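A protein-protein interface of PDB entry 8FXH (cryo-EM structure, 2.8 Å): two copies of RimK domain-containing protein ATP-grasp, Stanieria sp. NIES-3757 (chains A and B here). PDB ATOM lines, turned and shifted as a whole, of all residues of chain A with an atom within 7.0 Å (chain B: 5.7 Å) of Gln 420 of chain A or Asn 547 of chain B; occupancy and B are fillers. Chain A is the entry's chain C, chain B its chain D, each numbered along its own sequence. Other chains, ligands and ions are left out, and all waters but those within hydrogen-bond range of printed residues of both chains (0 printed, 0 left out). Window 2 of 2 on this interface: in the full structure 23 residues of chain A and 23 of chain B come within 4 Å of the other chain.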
ATOM      1  N   GLY A 314      31.296  15.022  -8.832  1.00  0.00           N
ATOM      2  CA  GLY A 314      30.242  15.504  -7.968  1.00  0.00           C
ATOM      3  C   GLY A 314      30.371  15.122  -6.513  1.00  0.00           C
ATOM      4  O   GLY A 314      29.407  15.292  -5.761  1.00  0.00           O
ATOM      5  N   LEU A 414      26.834  21.729   0.734  1.00  0.00           N
ATOM      6  CA  LEU A 414      26.855  22.923  -0.104  1.00  0.00           C
ATOM      7  C   LEU A 414      27.779  22.741  -1.302  1.00  0.00           C
ATOM      8  O   LEU A 414      27.437  23.128  -2.427  1.00  0.00           O
ATOM      9  CB  LEU A 414      27.283  24.128   0.727  1.00  0.00           C
ATOM     10  CG  LEU A 414      27.528  25.441  -0.013  1.00  0.00           C
ATOM     11  CD1 LEU A 414      26.216  26.121  -0.313  1.00  0.00           C
ATOM     12  CD2 LEU A 414      28.415  26.346   0.806  1.00  0.00           C
ATOM     13  N   ALA A 415      28.955  22.152  -1.080  1.00  0.00           N
ATOM     14  CA  ALA A 415      29.879  21.905  -2.180  1.00  0.00           C
ATOM     15  C   ALA A 415      29.286  20.942  -3.196  1.00  0.00           C
ATOM     16  O   ALA A 415      29.440  21.136  -4.407  1.00  0.00           O
ATOM     17  CB  ALA A 415      31.201  21.367  -1.642  1.00  0.00           C
ATOM     18  N   GLN A 416      28.610  19.891  -2.728  1.00  0.00           N
ATOM     19  CA  GLN A 416      27.974  18.958  -3.654  1.00  0.00           C
ATOM     20  C   GLN A 416      26.904  19.650  -4.489  1.00  0.00           C
ATOM     21  O   GLN A 416      26.809  19.423  -5.703  1.00  0.00           O
ATOM     22  CB  GLN A 416      27.368  17.784  -2.891  1.00  0.00           C
ATOM     23  CG  GLN A 416      28.377  16.857  -2.268  1.00  0.00           C
ATOM     24  CD  GLN A 416      27.728  15.751  -1.473  1.00  0.00           C
ATOM     25  OE1 GLN A 416      28.297  14.676  -1.308  1.00  0.00           O
ATOM     26  NE2 GLN A 416      26.532  16.011  -0.969  1.00  0.00           N
ATOM     27  N   ASP A 417      26.085  20.491  -3.856  1.00  0.00           N
ATOM     28  CA  ASP A 417      25.050  21.212  -4.591  1.00  0.00           C
ATOM     29  C   ASP A 417      25.652  22.145  -5.630  1.00  0.00           C
ATOM     30  O   ASP A 417      25.127  22.267  -6.740  1.00  0.00           O
ATOM     31  CB  ASP A 417      24.160  21.994  -3.627  1.00  0.00           C
ATOM     32  CG  ASP A 417      23.489  21.106  -2.604  1.00  0.00           C
ATOM     33  OD1 ASP A 417      23.835  19.909  -2.534  1.00  0.00           O
ATOM     34  OD2 ASP A 417      22.614  21.606  -1.866  1.00  0.00           O
ATOM     35  N   ILE A 418      26.744  22.827  -5.287  1.00  0.00           N
ATOM     36  CA  ILE A 418      27.397  23.699  -6.259  1.00  0.00           C
ATOM     37  C   ILE A 418      27.946  22.884  -7.423  1.00  0.00           C
ATOM     38  O   ILE A 418      27.789  23.253  -8.592  1.00  0.00           O
ATOM     39  CB  ILE A 418      28.505  24.527  -5.586  1.00  0.00           C
ATOM     40  CG1 ILE A 418      27.903  25.554  -4.637  1.00  0.00           C
ATOM     41  CG2 ILE A 418      29.348  25.225  -6.626  1.00  0.00           C
ATOM     42  CD1 ILE A 418      28.931  26.392  -3.941  1.00  0.00           C
ATOM     43  N   ALA A 419      28.595  21.758  -7.123  1.00  0.00           N
ATOM     44  CA  ALA A 419      29.293  21.001  -8.154  1.00  0.00           C
ATOM     45  C   ALA A 419      28.356  20.220  -9.060  1.00  0.00           C
ATOM     46  O   ALA A 419      28.748  19.882 -10.179  1.00  0.00           O
ATOM     47  CB  ALA A 419      30.293  20.043  -7.513  1.00  0.00           C
ATOM     48  N   GLN A 420      27.139  19.912  -8.613  1.00  0.00           N
ATOM     49  CA  GLN A 420      26.263  19.086  -9.436  1.00  0.00           C
ATOM     50  C   GLN A 420      25.715  19.812 -10.658  1.00  0.00           C
ATOM     51  O   GLN A 420      25.085  19.165 -11.499  1.00  0.00           O
ATOM     52  CB  GLN A 420      25.100  18.557  -8.601  1.00  0.00           C
ATOM     53  CG  GLN A 420      23.964  19.541  -8.440  1.00  0.00           C
ATOM     54  CD  GLN A 420      22.760  18.931  -7.762  1.00  0.00           C
ATOM     55  OE1 GLN A 420      22.669  17.715  -7.616  1.00  0.00           O
ATOM     56  NE2 GLN A 420      21.830  19.774  -7.338  1.00  0.00           N
ATOM     57  N   HIS A 421      25.924  21.118 -10.784  1.00  0.00           N
ATOM     58  CA  HIS A 421      25.302  21.903 -11.842  1.00  0.00           C
ATOM     59  C   HIS A 421      26.162  22.049 -13.091  1.00  0.00           C
ATOM     60  O   HIS A 421      25.734  22.719 -14.035  1.00  0.00           O
ATOM     61  CB  HIS A 421      24.941  23.295 -11.319  1.00  0.00           C
ATOM     62  CG  HIS A 421      23.629  23.348 -10.603  1.00  0.00           C
ATOM     63  ND1 HIS A 421      22.428  23.502 -11.260  1.00  0.00           N
ATOM     64  CD2 HIS A 421      23.328  23.268  -9.286  1.00  0.00           C
ATOM     65  CE1 HIS A 421      21.445  23.511 -10.380  1.00  0.00           C
ATOM     66  NE2 HIS A 421      21.964  23.372  -9.174  1.00  0.00           N
ATOM     67  N   PHE A 422      27.349  21.453 -13.133  1.00  0.00           N
ATOM     68  CA  PHE A 422      28.257  21.604 -14.259  1.00  0.00           C
ATOM     69  C   PHE A 422      28.633  20.243 -14.827  1.00  0.00           C
ATOM     70  O   PHE A 422      28.662  19.239 -14.111  1.00  0.00           O
ATOM     71  CB  PHE A 422      29.530  22.350 -13.855  1.00  0.00           C
ATOM     72  CG  PHE A 422      29.285  23.736 -13.344  1.00  0.00           C
ATOM     73  CD1 PHE A 422      29.096  24.785 -14.220  1.00  0.00           C
ATOM     74  CD2 PHE A 422      29.252  23.992 -11.988  1.00  0.00           C
ATOM     75  CE1 PHE A 422      28.876  26.061 -13.754  1.00  0.00           C
ATOM     76  CE2 PHE A 422      29.030  25.267 -11.517  1.00  0.00           C
ATOM     77  CZ  PHE A 422      28.843  26.302 -12.400  1.00  0.00           C
ATOM     78  N   ARG A 423      28.921  20.219 -16.123  1.00  0.00           N
ATOM     79  CA  ARG A 423      29.354  18.998 -16.803  1.00  0.00           C
ATOM     80  C   ARG A 423      30.878  18.952 -16.908  1.00  0.00           C
ATOM     81  O   ARG A 423      31.458  18.979 -17.988  1.00  0.00           O
ATOM     82  CB  ARG A 423      28.706  18.903 -18.180  1.00  0.00           C
ATOM     83  CG  ARG A 423      27.286  18.387 -18.159  1.00  0.00           C
ATOM     84  CD  ARG A 423      26.737  18.243 -19.563  1.00  0.00           C
ATOM     85  NE  ARG A 423      27.286  17.084 -20.253  1.00  0.00           N
ATOM     86  CZ  ARG A 423      26.616  15.964 -20.479  1.00  0.00           C
ATOM     87  NH1 ARG A 423      25.366  15.814 -20.077  1.00  0.00           N
ATOM     88  NH2 ARG A 423      27.215  14.968 -21.123  1.00  0.00           N
ATOM     89  N   LEU A 427      36.397  19.899 -10.203  1.00  0.00           N
ATOM     90  CA  LEU A 427      36.056  21.290  -9.948  1.00  0.00           C
ATOM     91  C   LEU A 427      36.753  21.764  -8.685  1.00  0.00           C
ATOM     92  O   LEU A 427      36.852  21.018  -7.707  1.00  0.00           O
ATOM     93  CB  LEU A 427      34.543  21.470  -9.808  1.00  0.00           C
ATOM     94  CG  LEU A 427      33.980  22.872 -10.037  1.00  0.00           C
ATOM     95  CD1 LEU A 427      34.109  23.270 -11.489  1.00  0.00           C
ATOM     96  CD2 LEU A 427      32.537  22.939  -9.600  1.00  0.00           C
ATOM     97  N   GLY B 192      14.056  18.657 -16.396  1.00  0.00           N
ATOM     98  CA  GLY B 192      14.759  17.842 -15.426  1.00  0.00           C
ATOM     99  C   GLY B 192      15.981  17.117 -15.945  1.00  0.00           C
ATOM    100  O   GLY B 192      16.911  17.742 -16.456  1.00  0.00           O
ATOM    101  N   LYS B 193      15.989  15.795 -15.814  1.00  0.00           N
ATOM    102  CA  LYS B 193      17.133  14.974 -16.177  1.00  0.00           C
ATOM    103  C   LYS B 193      17.171  14.630 -17.656  1.00  0.00           C
ATOM    104  O   LYS B 193      18.053  13.880 -18.083  1.00  0.00           O
ATOM    105  CB  LYS B 193      17.141  13.686 -15.354  1.00  0.00           C
ATOM    106  CG  LYS B 193      16.018  12.741 -15.695  1.00  0.00           C
ATOM    107  CD  LYS B 193      16.150  11.443 -14.935  1.00  0.00           C
ATOM    108  CE  LYS B 193      15.004  10.505 -15.257  1.00  0.00           C
ATOM    109  NZ  LYS B 193      15.125   9.917 -16.615  1.00  0.00           N
ATOM    110  N   GLN B 195      17.239  17.060 -20.109  1.00  0.00           N
ATOM    111  CA  GLN B 195      17.432  18.387 -20.663  1.00  0.00           C
ATOM    112  C   GLN B 195      18.590  18.421 -21.649  1.00  0.00           C
ATOM    113  O   GLN B 195      19.535  17.638 -21.554  1.00  0.00           O
ATOM    114  CB  GLN B 195      17.695  19.390 -19.544  1.00  0.00           C
ATOM    115  CG  GLN B 195      18.883  19.026 -18.683  1.00  0.00           C
ATOM    116  CD  GLN B 195      19.279  20.126 -17.733  1.00  0.00           C
ATOM    117  OE1 GLN B 195      20.285  20.801 -17.933  1.00  0.00           O
ATOM    118  NE2 GLN B 195      18.493  20.312 -16.687  1.00  0.00           N
ATOM    119  N   ILE B 526      13.850  19.441  -1.398  1.00  0.00           N
ATOM    120  CA  ILE B 526      14.415  18.392  -2.237  1.00  0.00           C
ATOM    121  C   ILE B 526      14.474  17.142  -1.374  1.00  0.00           C
ATOM    122  O   ILE B 526      15.198  17.110  -0.372  1.00  0.00           O
ATOM    123  CB  ILE B 526      15.799  18.760  -2.780  1.00  0.00           C
ATOM    124  CG1 ILE B 526      15.673  19.784  -3.904  1.00  0.00           C
ATOM    125  CG2 ILE B 526      16.511  17.526  -3.283  1.00  0.00           C
ATOM    126  CD1 ILE B 526      16.989  20.178  -4.511  1.00  0.00           C
ATOM    127  N   LEU B 542      11.696  27.666 -12.108  1.00  0.00           N
ATOM    128  CA  LEU B 542      12.775  27.622 -13.088  1.00  0.00           C
ATOM    129  C   LEU B 542      14.015  26.964 -12.506  1.00  0.00           C
ATOM    130  O   LEU B 542      14.690  26.185 -13.185  1.00  0.00           O
ATOM    131  CB  LEU B 542      13.098  29.034 -13.573  1.00  0.00           C
ATOM    132  CG  LEU B 542      14.087  29.181 -14.731  1.00  0.00           C
ATOM    133  CD1 LEU B 542      13.650  30.293 -15.654  1.00  0.00           C
ATOM    134  CD2 LEU B 542      15.487  29.456 -14.221  1.00  0.00           C
ATOM    135  N   ASN B 543      14.340  27.277 -11.251  1.00  0.00           N
ATOM    136  CA  ASN B 543      15.497  26.663 -10.611  1.00  0.00           C
ATOM    137  C   ASN B 543      15.315  25.159 -10.471  1.00  0.00           C
ATOM    138  O   ASN B 543      16.274  24.395 -10.619  1.00  0.00           O
ATOM    139  CB  ASN B 543      15.741  27.299  -9.246  1.00  0.00           C
ATOM    140  CG  ASN B 543      16.399  28.653  -9.347  1.00  0.00           C
ATOM    141  OD1 ASN B 543      16.778  29.091 -10.430  1.00  0.00           O
ATOM    142  ND2 ASN B 543      16.535  29.328  -8.215  1.00  0.00           N
ATOM    143  N   LEU B 544      14.098  24.716 -10.162  1.00  0.00           N
ATOM    144  CA  LEU B 544      13.857  23.286 -10.010  1.00  0.00           C
ATOM    145  C   LEU B 544      13.912  22.561 -11.348  1.00  0.00           C
ATOM    146  O   LEU B 544      14.455  21.457 -11.436  1.00  0.00           O
ATOM    147  CB  LEU B 544      12.513  23.046  -9.328  1.00  0.00           C
ATOM    148  CG  LEU B 544      12.506  23.163  -7.807  1.00  0.00           C
ATOM    149  CD1 LEU B 544      11.097  23.049  -7.283  1.00  0.00           C
ATOM    150  CD2 LEU B 544      13.389  22.107  -7.189  1.00  0.00           C
ATOM    151  N   LEU B 545      13.351  23.158 -12.401  1.00  0.00           N
ATOM    152  CA  LEU B 545      13.366  22.510 -13.708  1.00  0.00           C
ATOM    153  C   LEU B 545      14.744  22.501 -14.354  1.00  0.00           C
ATOM    154  O   LEU B 545      14.953  21.754 -15.313  1.00  0.00           O
ATOM    155  CB  LEU B 545      12.372  23.186 -14.649  1.00  0.00           C
ATOM    156  CG  LEU B 545      10.891  22.902 -14.409  1.00  0.00           C
ATOM    157  CD1 LEU B 545      10.039  23.735 -15.338  1.00  0.00           C
ATOM    158  CD2 LEU B 545      10.596  21.432 -14.586  1.00  0.00           C
ATOM    159  N   ARG B 546      15.677  23.313 -13.867  1.00  0.00           N
ATOM    160  CA  ARG B 546      17.042  23.338 -14.375  1.00  0.00           C
ATOM    161  C   ARG B 546      17.918  22.251 -13.761  1.00  0.00           C
ATOM    162  O   ARG B 546      18.951  21.906 -14.341  1.00  0.00           O
ATOM    163  CB  ARG B 546      17.642  24.729 -14.123  1.00  0.00           C
ATOM    164  CG  ARG B 546      19.144  24.859 -14.276  1.00  0.00           C
ATOM    165  CD  ARG B 546      19.560  24.878 -15.728  1.00  0.00           C
ATOM    166  NE  ARG B 546      20.971  25.201 -15.884  1.00  0.00           N
ATOM    167  CZ  ARG B 546      21.961  24.338 -15.715  1.00  0.00           C
ATOM    168  NH1 ARG B 546      21.731  23.079 -15.389  1.00  0.00           N
ATOM    169  NH2 ARG B 546      23.214  24.748 -15.882  1.00  0.00           N
ATOM    170  N   ASN B 547      17.509  21.674 -12.639  1.00  0.00           N
ATOM    171  CA  ASN B 547      18.286  20.643 -11.964  1.00  0.00           C
ATOM    172  C   ASN B 547      18.443  19.420 -12.859  1.00  0.00           C
ATOM    173  O   ASN B 547      17.436  18.869 -13.320  1.00  0.00           O
ATOM    174  CB  ASN B 547      17.600  20.250 -10.661  1.00  0.00           C
ATOM    175  CG  ASN B 547      18.543  19.607  -9.675  1.00  0.00           C
ATOM    176  OD1 ASN B 547      19.313  18.719 -10.024  1.00  0.00           O
ATOM    177  ND2 ASN B 547      18.480  20.046  -8.429  1.00  0.00           N
ATOM    178  N   PRO B 548      19.667  18.959 -13.120  1.00  0.00           N
ATOM    179  CA  PRO B 548      19.866  17.825 -14.028  1.00  0.00           C
ATOM    180  C   PRO B 548      19.659  16.458 -13.400  1.00  0.00           C
ATOM    181  O   PRO B 548      20.047  15.459 -14.009  1.00  0.00           O
ATOM    182  CB  PRO B 548      21.326  18.000 -14.464  1.00  0.00           C
ATOM    183  CG  PRO B 548      21.968  18.669 -13.326  1.00  0.00           C
ATOM    184  CD  PRO B 548      20.942  19.559 -12.697  1.00  0.00           C
ATOM    185  N   LYS B 549      19.067  16.375 -12.209  1.00  0.00           N
ATOM    186  CA  LYS B 549      18.809  15.094 -11.573  1.00  0.00           C
ATOM    187  C   LYS B 549      17.363  14.907 -11.146  1.00  0.00           C
ATOM    188  O   LYS B 549      17.053  13.887 -10.525  1.00  0.00           O
ATOM    189  CB  LYS B 549      19.716  14.911 -10.348  1.00  0.00           C
ATOM    190  CG  LYS B 549      21.175  15.230 -10.596  1.00  0.00           C
ATOM    191  CD  LYS B 549      22.087  14.226  -9.920  1.00  0.00           C
ATOM    192  CE  LYS B 549      21.789  14.127  -8.438  1.00  0.00           C
ATOM    193  NZ  LYS B 549      22.591  13.061  -7.781  1.00  0.00           N
ATOM    194  N   LEU B 550      16.476  15.846 -11.454  1.00  0.00           N
ATOM    195  CA  LEU B 550      15.103  15.767 -10.978  1.00  0.00           C
ATOM    196  C   LEU B 550      14.353  14.627 -11.653  1.00  0.00           C
ATOM    197  O   LEU B 550      14.574  14.324 -12.826  1.00  0.00           O
ATOM    198  CB  LEU B 550      14.379  17.084 -11.231  1.00  0.00           C
ATOM    199  CG  LEU B 550      13.414  17.543 -10.142  1.00  0.00           C
ATOM    200  CD1 LEU B 550      14.176  18.166  -9.001  1.00  0.00           C
ATOM    201  CD2 LEU B 550      12.416  18.522 -10.709  1.00  0.00           C
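No position is printed for both chains. Of the 4 pairs that touch across the chains among the printed residues, none has its exchanged pair printed and touching as well.
Asn 547 of chain B touches Gln 420 of chain A (ND2 to NE2, 3.5 Å). Gln 420 of chain A touches Pro 548 of chain B (O to CG, 3.6 Å). OE1 of Gln 420 of chain A touches CE of Lys 549 of chain B, at 3.8 Å. NH2 of Arg 546 of chain B touches O of His 421 of chain A (3.7 Å).
The side-chain amide nitrogen of Gln 195 of chain B lies within hydrogen-bond range of the backbone carbonyl oxygen of Arg 546 of chain B. The backbone NH (N) of Lys 549 of chain B lies close to the side-chain amide oxygen (OD1) of Asn 547 of chain B, 3.2 Å away.
Of the 13 printed residues of chain B, 4 touch a printed residue of chain A. Hydrophobic or aromatic side chains of chain B that line the printed part of chain A: Pro 548. Of the 12 printed residues of chain A, 2 touch a printed residue of chain B. Among the printed residues, 4 pairs touch across the chains.
Of chain B, only Asn 547, Pro 548 and Lys 549 come within 4 Å of Gln 420 of chain A. Asn 547 of chain B touches just one residue of chain A: Gln 420 (3.5 Å). Of the printed residues of chain A, Arg 546 of chain B touches His 421. Of the printed residues of chain B, His 421 of chain A touches Arg 546. Of the printed residues of chain A, Lys 549 of chain B touches Gln 420. Leu 542 of chain B touches none of the printed residues of chain A. Phe 422 of chain A touches none of the printed residues of chain B. The nearest residue of chain B that does not touch Gln 420 of chain A is Ile 526 of chain B (5.6 Å). The nearest printed residue of chain A that does not touch Lys 549 of chain B is Gly 314 of chain A (7.5 Å).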
